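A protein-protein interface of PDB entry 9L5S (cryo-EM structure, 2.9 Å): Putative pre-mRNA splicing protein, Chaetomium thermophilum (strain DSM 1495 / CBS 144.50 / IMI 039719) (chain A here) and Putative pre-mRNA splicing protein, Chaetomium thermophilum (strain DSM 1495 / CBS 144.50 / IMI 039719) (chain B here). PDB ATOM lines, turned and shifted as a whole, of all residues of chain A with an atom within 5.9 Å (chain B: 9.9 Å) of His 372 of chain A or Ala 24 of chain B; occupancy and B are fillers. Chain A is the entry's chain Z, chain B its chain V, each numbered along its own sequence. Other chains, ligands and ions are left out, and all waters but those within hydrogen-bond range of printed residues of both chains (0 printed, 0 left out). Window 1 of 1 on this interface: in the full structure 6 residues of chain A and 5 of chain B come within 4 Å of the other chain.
The backbone NH (N) of Leu 23 of chain B sits at hydrogen-bond distance from a ring nitrogen (ND1) of His 372 of chain A (3.4 Å).
The side-chain amide oxygen of Gln 20 of chain B lies within hydrogen-bond range of a ring nitrogen (NE2) of His 372 of chain A.
The side-chain amino group (NZ) of Lys 376 of chain A lies close to the side-chain amide nitrogen (NE2) of Gln 20 of chain B (3.0 Å).
Of the printed residues of chain B, Glu 368 of chain A touches Asn 22 (3.98 Å) and Ala 24 (3.8 Å).
No residue of chain B comes within 4 Å of Ala 370 of chain A.
Of chain B, only Ala 24 (3.8 Å) comes within 4 Å of Ala 371 of chain A.
His 372 of chain A touches four residues of chain B.
Of the printed residues of chain B, Lys 376 of chain A touches Gln 20 (3.0 Å).
Val 19 of chain B touches none of the printed residues of chain A.
Of the printed residues of chain A, Gln 20 of chain B touches His 372 and Lys 376.
Of the printed residues of chain A, Asn 22 of chain B touches Glu 368 and His 372.
Of the printed residues of chain A, Leu 23 of chain B touches His 372 (3.4 Å) and Met 375 (3.6 Å).
Ala 24 of chain B touches four residues of chain A.
Leu 26 of chain B touches none of the printed residues of chain A.
The nearest printed residue of chain A that does not touch Gln 20 of chain B is Lys 373 of chain A (6.1 Å).
Among the printed residues, pairs that only touch across the chains: His 372 of chain A with Ala 24 of chain B (3.5 Å), Met 375 of chain A with Leu 23 of chain B (3.6 Å), His 372 of chain A with Asn 22 of chain B (3.8 Å), Ala 371 of chain A with Ala 24 of chain B (3.8 Å), Glu 368 of chain A with Ala 24 of chain B (3.8 Å), Met 375 of chain A with Ala 24 of chain B (3.8 Å) and Glu 368 of chain A with Asn 22 of chain B (3.98 Å).
Of the 11 printed residues of chain A, 5 touch a printed residue of chain B.
Hydrophobic or aromatic side chains of chain A within 4 Å of the printed part of chain B: Ala 371, His 372 and Met 375.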
ATOM      1  N   GLU A 368       5.909  11.792  -6.781  1.00  0.00           N
ATOM      2  CA  GLU A 368       6.560  10.574  -6.318  1.00  0.00           C
ATOM      3  C   GLU A 368       6.767  10.745  -4.822  1.00  0.00           C
ATOM      4  O   GLU A 368       6.784   9.775  -4.057  1.00  0.00           O
ATOM      5  CB  GLU A 368       7.900  10.341  -7.022  1.00  0.00           C
ATOM      6  CG  GLU A 368       7.860  10.387  -8.540  1.00  0.00           C
ATOM      7  CD  GLU A 368       8.857   9.438  -9.176  1.00  0.00           C
ATOM      8  OE1 GLU A 368       9.354   8.537  -8.469  1.00  0.00           O
ATOM      9  OE2 GLU A 368       9.144   9.593 -10.382  1.00  0.00           O
ATOM     10  N   GLU A 369       6.926  12.007  -4.417  1.00  0.00           N
ATOM     11  CA  GLU A 369       7.067  12.360  -3.009  1.00  0.00           C
ATOM     12  C   GLU A 369       5.762  12.151  -2.254  1.00  0.00           C
ATOM     13  O   GLU A 369       5.769  11.699  -1.101  1.00  0.00           O
ATOM     14  CB  GLU A 369       7.535  13.812  -2.909  1.00  0.00           C
ATOM     15  CG  GLU A 369       7.851  14.320  -1.519  1.00  0.00           C
ATOM     16  CD  GLU A 369       7.767  15.834  -1.445  1.00  0.00           C
ATOM     17  OE1 GLU A 369       8.124  16.494  -2.444  1.00  0.00           O
ATOM     18  OE2 GLU A 369       7.345  16.366  -0.400  1.00  0.00           O
ATOM     19  N   ALA A 370       4.633  12.474  -2.892  1.00  0.00           N
ATOM     20  CA  ALA A 370       3.330  12.302  -2.258  1.00  0.00           C
ATOM     21  C   ALA A 370       3.032  10.831  -2.002  1.00  0.00           C
ATOM     22  O   ALA A 370       2.568  10.466  -0.918  1.00  0.00           O
ATOM     23  CB  ALA A 370       2.238  12.930  -3.124  1.00  0.00           C
ATOM     24  N   ALA A 371       3.310   9.968  -2.985  1.00  0.00           N
ATOM     25  CA  ALA A 371       3.104   8.534  -2.804  1.00  0.00           C
ATOM     26  C   ALA A 371       4.037   7.970  -1.742  1.00  0.00           C
ATOM     27  O   ALA A 371       3.639   7.108  -0.947  1.00  0.00           O
ATOM     28  CB  ALA A 371       3.304   7.803  -4.132  1.00  0.00           C
ATOM     29  N   HIS A 372       5.288   8.440  -1.725  1.00  0.00           N
ATOM     30  CA  HIS A 372       6.256   7.977  -0.739  1.00  0.00           C
ATOM     31  C   HIS A 372       5.824   8.343   0.676  1.00  0.00           C
ATOM     32  O   HIS A 372       5.930   7.522   1.594  1.00  0.00           O
ATOM     33  CB  HIS A 372       7.637   8.555  -1.062  1.00  0.00           C
ATOM     34  CG  HIS A 372       8.561   8.627   0.114  1.00  0.00           C
ATOM     35  ND1 HIS A 372       9.397   7.589   0.464  1.00  0.00           N
ATOM     36  CD2 HIS A 372       8.808   9.622   0.998  1.00  0.00           C
ATOM     37  CE1 HIS A 372      10.103   7.932   1.526  1.00  0.00           C
ATOM     38  NE2 HIS A 372       9.764   9.162   1.870  1.00  0.00           N
ATOM     39  N   LYS A 373       5.329   9.566   0.873  1.00  0.00           N
ATOM     40  CA  LYS A 373       4.880   9.955   2.205  1.00  0.00           C
ATOM     41  C   LYS A 373       3.517   9.365   2.558  1.00  0.00           C
ATOM     42  O   LYS A 373       3.198   9.237   3.744  1.00  0.00           O
ATOM     43  CB  LYS A 373       4.848  11.477   2.333  1.00  0.00           C
ATOM     44  CG  LYS A 373       6.222  12.120   2.319  1.00  0.00           C
ATOM     45  CD  LYS A 373       6.150  13.582   2.715  1.00  0.00           C
ATOM     46  CE  LYS A 373       5.631  14.433   1.576  1.00  0.00           C
ATOM     47  NZ  LYS A 373       5.819  15.885   1.843  1.00  0.00           N
ATOM     48  N   LEU A 374       2.702   9.008   1.561  1.00  0.00           N
ATOM     49  CA  LEU A 374       1.434   8.350   1.861  1.00  0.00           C
ATOM     50  C   LEU A 374       1.632   6.890   2.244  1.00  0.00           C
ATOM     51  O   LEU A 374       0.880   6.364   3.072  1.00  0.00           O
ATOM     52  CB  LEU A 374       0.476   8.464   0.673  1.00  0.00           C
ATOM     53  CG  LEU A 374      -0.279   9.781   0.489  1.00  0.00           C
ATOM     54  CD1 LEU A 374      -0.918   9.838  -0.889  1.00  0.00           C
ATOM     55  CD2 LEU A 374      -1.328   9.958   1.572  1.00  0.00           C
ATOM     56  N   MET A 375       2.626   6.219   1.657  1.00  0.00           N
ATOM     57  CA  MET A 375       2.934   4.857   2.078  1.00  0.00           C
ATOM     58  C   MET A 375       3.575   4.812   3.459  1.00  0.00           C
ATOM     59  O   MET A 375       3.507   3.776   4.127  1.00  0.00           O
ATOM     60  CB  MET A 375       3.862   4.178   1.073  1.00  0.00           C
ATOM     61  CG  MET A 375       3.244   3.850  -0.274  1.00  0.00           C
ATOM     62  SD  MET A 375       4.535   3.722  -1.527  1.00  0.00           S
ATOM     63  CE  MET A 375       3.580   3.782  -3.039  1.00  0.00           C
ATOM     64  N   LYS A 376       4.193   5.909   3.899  1.00  0.00           N
ATOM     65  CA  LYS A 376       4.780   5.986   5.230  1.00  0.00           C
ATOM     66  C   LYS A 376       3.747   6.200   6.325  1.00  0.00           C
ATOM     67  O   LYS A 376       4.098   6.102   7.506  1.00  0.00           O
ATOM     68  CB  LYS A 376       5.813   7.113   5.292  1.00  0.00           C
ATOM     69  CG  LYS A 376       7.114   6.830   4.567  1.00  0.00           C
ATOM     70  CD  LYS A 376       8.152   7.870   4.943  1.00  0.00           C
ATOM     71  CE  LYS A 376       8.511   7.768   6.416  1.00  0.00           C
ATOM     72  NZ  LYS A 376       9.554   8.749   6.811  1.00  0.00           N
ATOM     73  N   LEU A 377       2.503   6.509   5.967  1.00  0.00           N
ATOM     74  CA  LEU A 377       1.460   6.706   6.963  1.00  0.00           C
ATOM     75  C   LEU A 377       1.141   5.387   7.656  1.00  0.00           C
ATOM     76  O   LEU A 377       0.849   4.384   6.999  1.00  0.00           O
ATOM     77  CB  LEU A 377       0.204   7.274   6.305  1.00  0.00           C
ATOM     78  CG  LEU A 377       0.210   8.770   5.989  1.00  0.00           C
ATOM     79  CD1 LEU A 377      -1.052   9.168   5.243  1.00  0.00           C
ATOM     80  CD2 LEU A 377       0.356   9.581   7.260  1.00  0.00           C
ATOM     81  N   LYS A 411       0.903   5.133  -9.075  1.00  0.00           N
ATOM     82  CA  LYS A 411       1.877   4.501  -8.191  1.00  0.00           C
ATOM     83  C   LYS A 411       1.212   3.728  -7.062  1.00  0.00           C
ATOM     84  O   LYS A 411       1.858   2.877  -6.443  1.00  0.00           O
ATOM     85  CB  LYS A 411       2.842   5.546  -7.638  1.00  0.00           C
ATOM     86  CG  LYS A 411       3.795   6.064  -8.692  1.00  0.00           C
ATOM     87  CD  LYS A 411       4.593   7.251  -8.208  1.00  0.00           C
ATOM     88  CE  LYS A 411       5.388   7.843  -9.353  1.00  0.00           C
ATOM     89  NZ  LYS A 411       4.516   8.553 -10.325  1.00  0.00           N
ATOM     90  N   TYR B  18      18.397  14.319   6.000  1.00  0.00           N
ATOM     91  CA  TYR B  18      18.072  12.911   6.217  1.00  0.00           C
ATOM     92  C   TYR B  18      17.663  12.318   4.874  1.00  0.00           C
ATOM     93  O   TYR B  18      16.696  12.765   4.251  1.00  0.00           O
ATOM     94  CB  TYR B  18      16.963  12.784   7.255  1.00  0.00           C
ATOM     95  CG  TYR B  18      16.502  11.372   7.523  1.00  0.00           C
ATOM     96  CD1 TYR B  18      17.389  10.402   7.971  1.00  0.00           C
ATOM     97  CD2 TYR B  18      15.175  11.010   7.329  1.00  0.00           C
ATOM     98  CE1 TYR B  18      16.965   9.110   8.220  1.00  0.00           C
ATOM     99  CE2 TYR B  18      14.742   9.723   7.574  1.00  0.00           C
ATOM    100  CZ  TYR B  18      15.640   8.776   8.019  1.00  0.00           C
ATOM    101  OH  TYR B  18      15.213   7.492   8.264  1.00  0.00           O
ATOM    102  N   VAL B  19      18.401  11.309   4.422  1.00  0.00           N
ATOM    103  CA  VAL B  19      18.179  10.722   3.106  1.00  0.00           C
ATOM    104  C   VAL B  19      17.348   9.454   3.255  1.00  0.00           C
ATOM    105  O   VAL B  19      17.576   8.644   4.162  1.00  0.00           O
ATOM    106  CB  VAL B  19      19.525  10.438   2.413  1.00  0.00           C
ATOM    107  CG1 VAL B  19      19.320   9.853   1.019  1.00  0.00           C
ATOM    108  CG2 VAL B  19      20.359  11.707   2.337  1.00  0.00           C
ATOM    109  N   GLN B  20      16.376   9.282   2.365  1.00  0.00           N
ATOM    110  CA  GLN B  20      15.516   8.111   2.346  1.00  0.00           C
ATOM    111  C   GLN B  20      15.648   7.403   1.003  1.00  0.00           C
ATOM    112  O   GLN B  20      16.214   7.934   0.043  1.00  0.00           O
ATOM    113  CB  GLN B  20      14.058   8.497   2.615  1.00  0.00           C
ATOM    114  CG  GLN B  20      13.791   8.878   4.059  1.00  0.00           C
ATOM    115  CD  GLN B  20      12.456   9.563   4.248  1.00  0.00           C
ATOM    116  OE1 GLN B  20      11.784   9.919   3.281  1.00  0.00           O
ATOM    117  NE2 GLN B  20      12.072   9.773   5.499  1.00  0.00           N
ATOM    118  N   ARG B  21      15.106   6.192   0.941  1.00  0.00           N
ATOM    119  CA  ARG B  21      15.263   5.321  -0.214  1.00  0.00           C
ATOM    120  C   ARG B  21      14.273   5.649  -1.330  1.00  0.00           C
ATOM    121  O   ARG B  21      14.434   5.146  -2.450  1.00  0.00           O
ATOM    122  CB  ARG B  21      15.122   3.854   0.239  1.00  0.00           C
ATOM    123  CG  ARG B  21      15.528   2.777  -0.771  1.00  0.00           C
ATOM    124  CD  ARG B  21      15.570   1.398  -0.136  1.00  0.00           C
ATOM    125  NE  ARG B  21      16.868   1.112   0.460  1.00  0.00           N
ATOM    126  CZ  ARG B  21      17.152   0.008   1.140  1.00  0.00           C
ATOM    127  NH1 ARG B  21      16.246  -0.935   1.333  1.00  0.00           N
ATOM    128  NH2 ARG B  21      18.375  -0.150   1.637  1.00  0.00           N
ATOM    129  N   ASN B  22      13.298   6.523  -1.062  1.00  0.00           N
ATOM    130  CA  ASN B  22      12.182   6.824  -1.964  1.00  0.00           C
ATOM    131  C   ASN B  22      11.420   5.537  -2.294  1.00  0.00           C
ATOM    132  O   ASN B  22      11.393   5.052  -3.422  1.00  0.00           O
ATOM    133  CB  ASN B  22      12.650   7.559  -3.229  1.00  0.00           C
ATOM    134  CG  ASN B  22      11.496   8.045  -4.097  1.00  0.00           C
ATOM    135  OD1 ASN B  22      10.332   8.004  -3.696  1.00  0.00           O
ATOM    136  ND2 ASN B  22      11.819   8.498  -5.304  1.00  0.00           N
ATOM    137  N   LEU B  23      10.809   4.987  -1.248  1.00  0.00           N
ATOM    138  CA  LEU B  23      10.128   3.693  -1.277  1.00  0.00           C
ATOM    139  C   LEU B  23       8.849   3.671  -2.160  1.00  0.00           C
ATOM    140  O   LEU B  23       8.167   2.637  -2.179  1.00  0.00           O
ATOM    141  CB  LEU B  23       9.837   3.259   0.166  1.00  0.00           C
ATOM    142  CG  LEU B  23       8.949   4.063   1.129  1.00  0.00           C
ATOM    143  CD1 LEU B  23       7.470   3.787   0.958  1.00  0.00           C
ATOM    144  CD2 LEU B  23       9.365   3.798   2.570  1.00  0.00           C
ATOM    145  N   ALA B  24       8.505   4.742  -2.874  1.00  0.00           N
ATOM    146  CA  ALA B  24       7.494   4.699  -3.919  1.00  0.00           C
ATOM    147  C   ALA B  24       8.099   4.536  -5.307  1.00  0.00           C
ATOM    148  O   ALA B  24       7.365   4.581  -6.299  1.00  0.00           O
ATOM    149  CB  ALA B  24       6.630   5.964  -3.880  1.00  0.00           C
ATOM    150  N   HIS B  25       9.416   4.355  -5.399  1.00  0.00           N
ATOM    151  CA  HIS B  25      10.069   4.140  -6.686  1.00  0.00           C
ATOM    152  C   HIS B  25       9.808   2.719  -7.164  1.00  0.00           C
ATOM    153  O   HIS B  25      10.043   1.754  -6.427  1.00  0.00           O
ATOM    154  CB  HIS B  25      11.568   4.400  -6.576  1.00  0.00           C
ATOM    155  CG  HIS B  25      12.374   3.760  -7.663  1.00  0.00           C
ATOM    156  ND1 HIS B  25      12.284   4.149  -8.982  1.00  0.00           N
ATOM    157  CD2 HIS B  25      13.288   2.763  -7.626  1.00  0.00           C
ATOM    158  CE1 HIS B  25      13.107   3.416  -9.712  1.00  0.00           C
ATOM    159  NE2 HIS B  25      13.728   2.567  -8.912  1.00  0.00           N
ATOM    160  N   LEU B  26       9.324   2.591  -8.395  1.00  0.00           N
ATOM    161  CA  LEU B  26       8.980   1.291  -8.956  1.00  0.00           C
ATOM    162  C   LEU B  26      10.251   0.525  -9.298  1.00  0.00           C
ATOM    163  O   LEU B  26      11.054   0.975 -10.122  1.00  0.00           O
ATOM    164  CB  LEU B  26       8.102   1.465 -10.193  1.00  0.00           C
ATOM    165  CG  LEU B  26       6.871   2.356 -10.009  1.00  0.00           C
ATOM    166  CD1 LEU B  26       6.128   2.531 -11.325  1.00  0.00           C
ATOM    167  CD2 LEU B  26       5.952   1.800  -8.933  1.00  0.00           C
ATOM    168  N   ARG B  27      10.433  -0.628  -8.657  1.00  0.00           N
ATOM    169  CA  ARG B  27      11.576  -1.480  -8.939  1.00  0.00           C
ATOM    170  C   ARG B  27      11.458  -2.073 -10.345  1.00  0.00           C
ATOM    171  O   ARG B  27      10.358  -2.146 -10.900  1.00  0.00           O
ATOM    172  CB  ARG B  27      11.673  -2.591  -7.892  1.00  0.00           C
ATOM    173  CG  ARG B  27      11.959  -2.080  -6.490  1.00  0.00           C
ATOM    174  CD  ARG B  27      12.096  -3.216  -5.491  1.00  0.00           C
ATOM    175  NE  ARG B  27      12.530  -2.736  -4.185  1.00  0.00           N
ATOM    176  CZ  ARG B  27      11.725  -2.554  -3.147  1.00  0.00           C
ATOM    177  NH1 ARG B  27      10.428  -2.799  -3.229  1.00  0.00           N
ATOM    178  NH2 ARG B  27      12.233  -2.115  -2.000  1.00  0.00           N
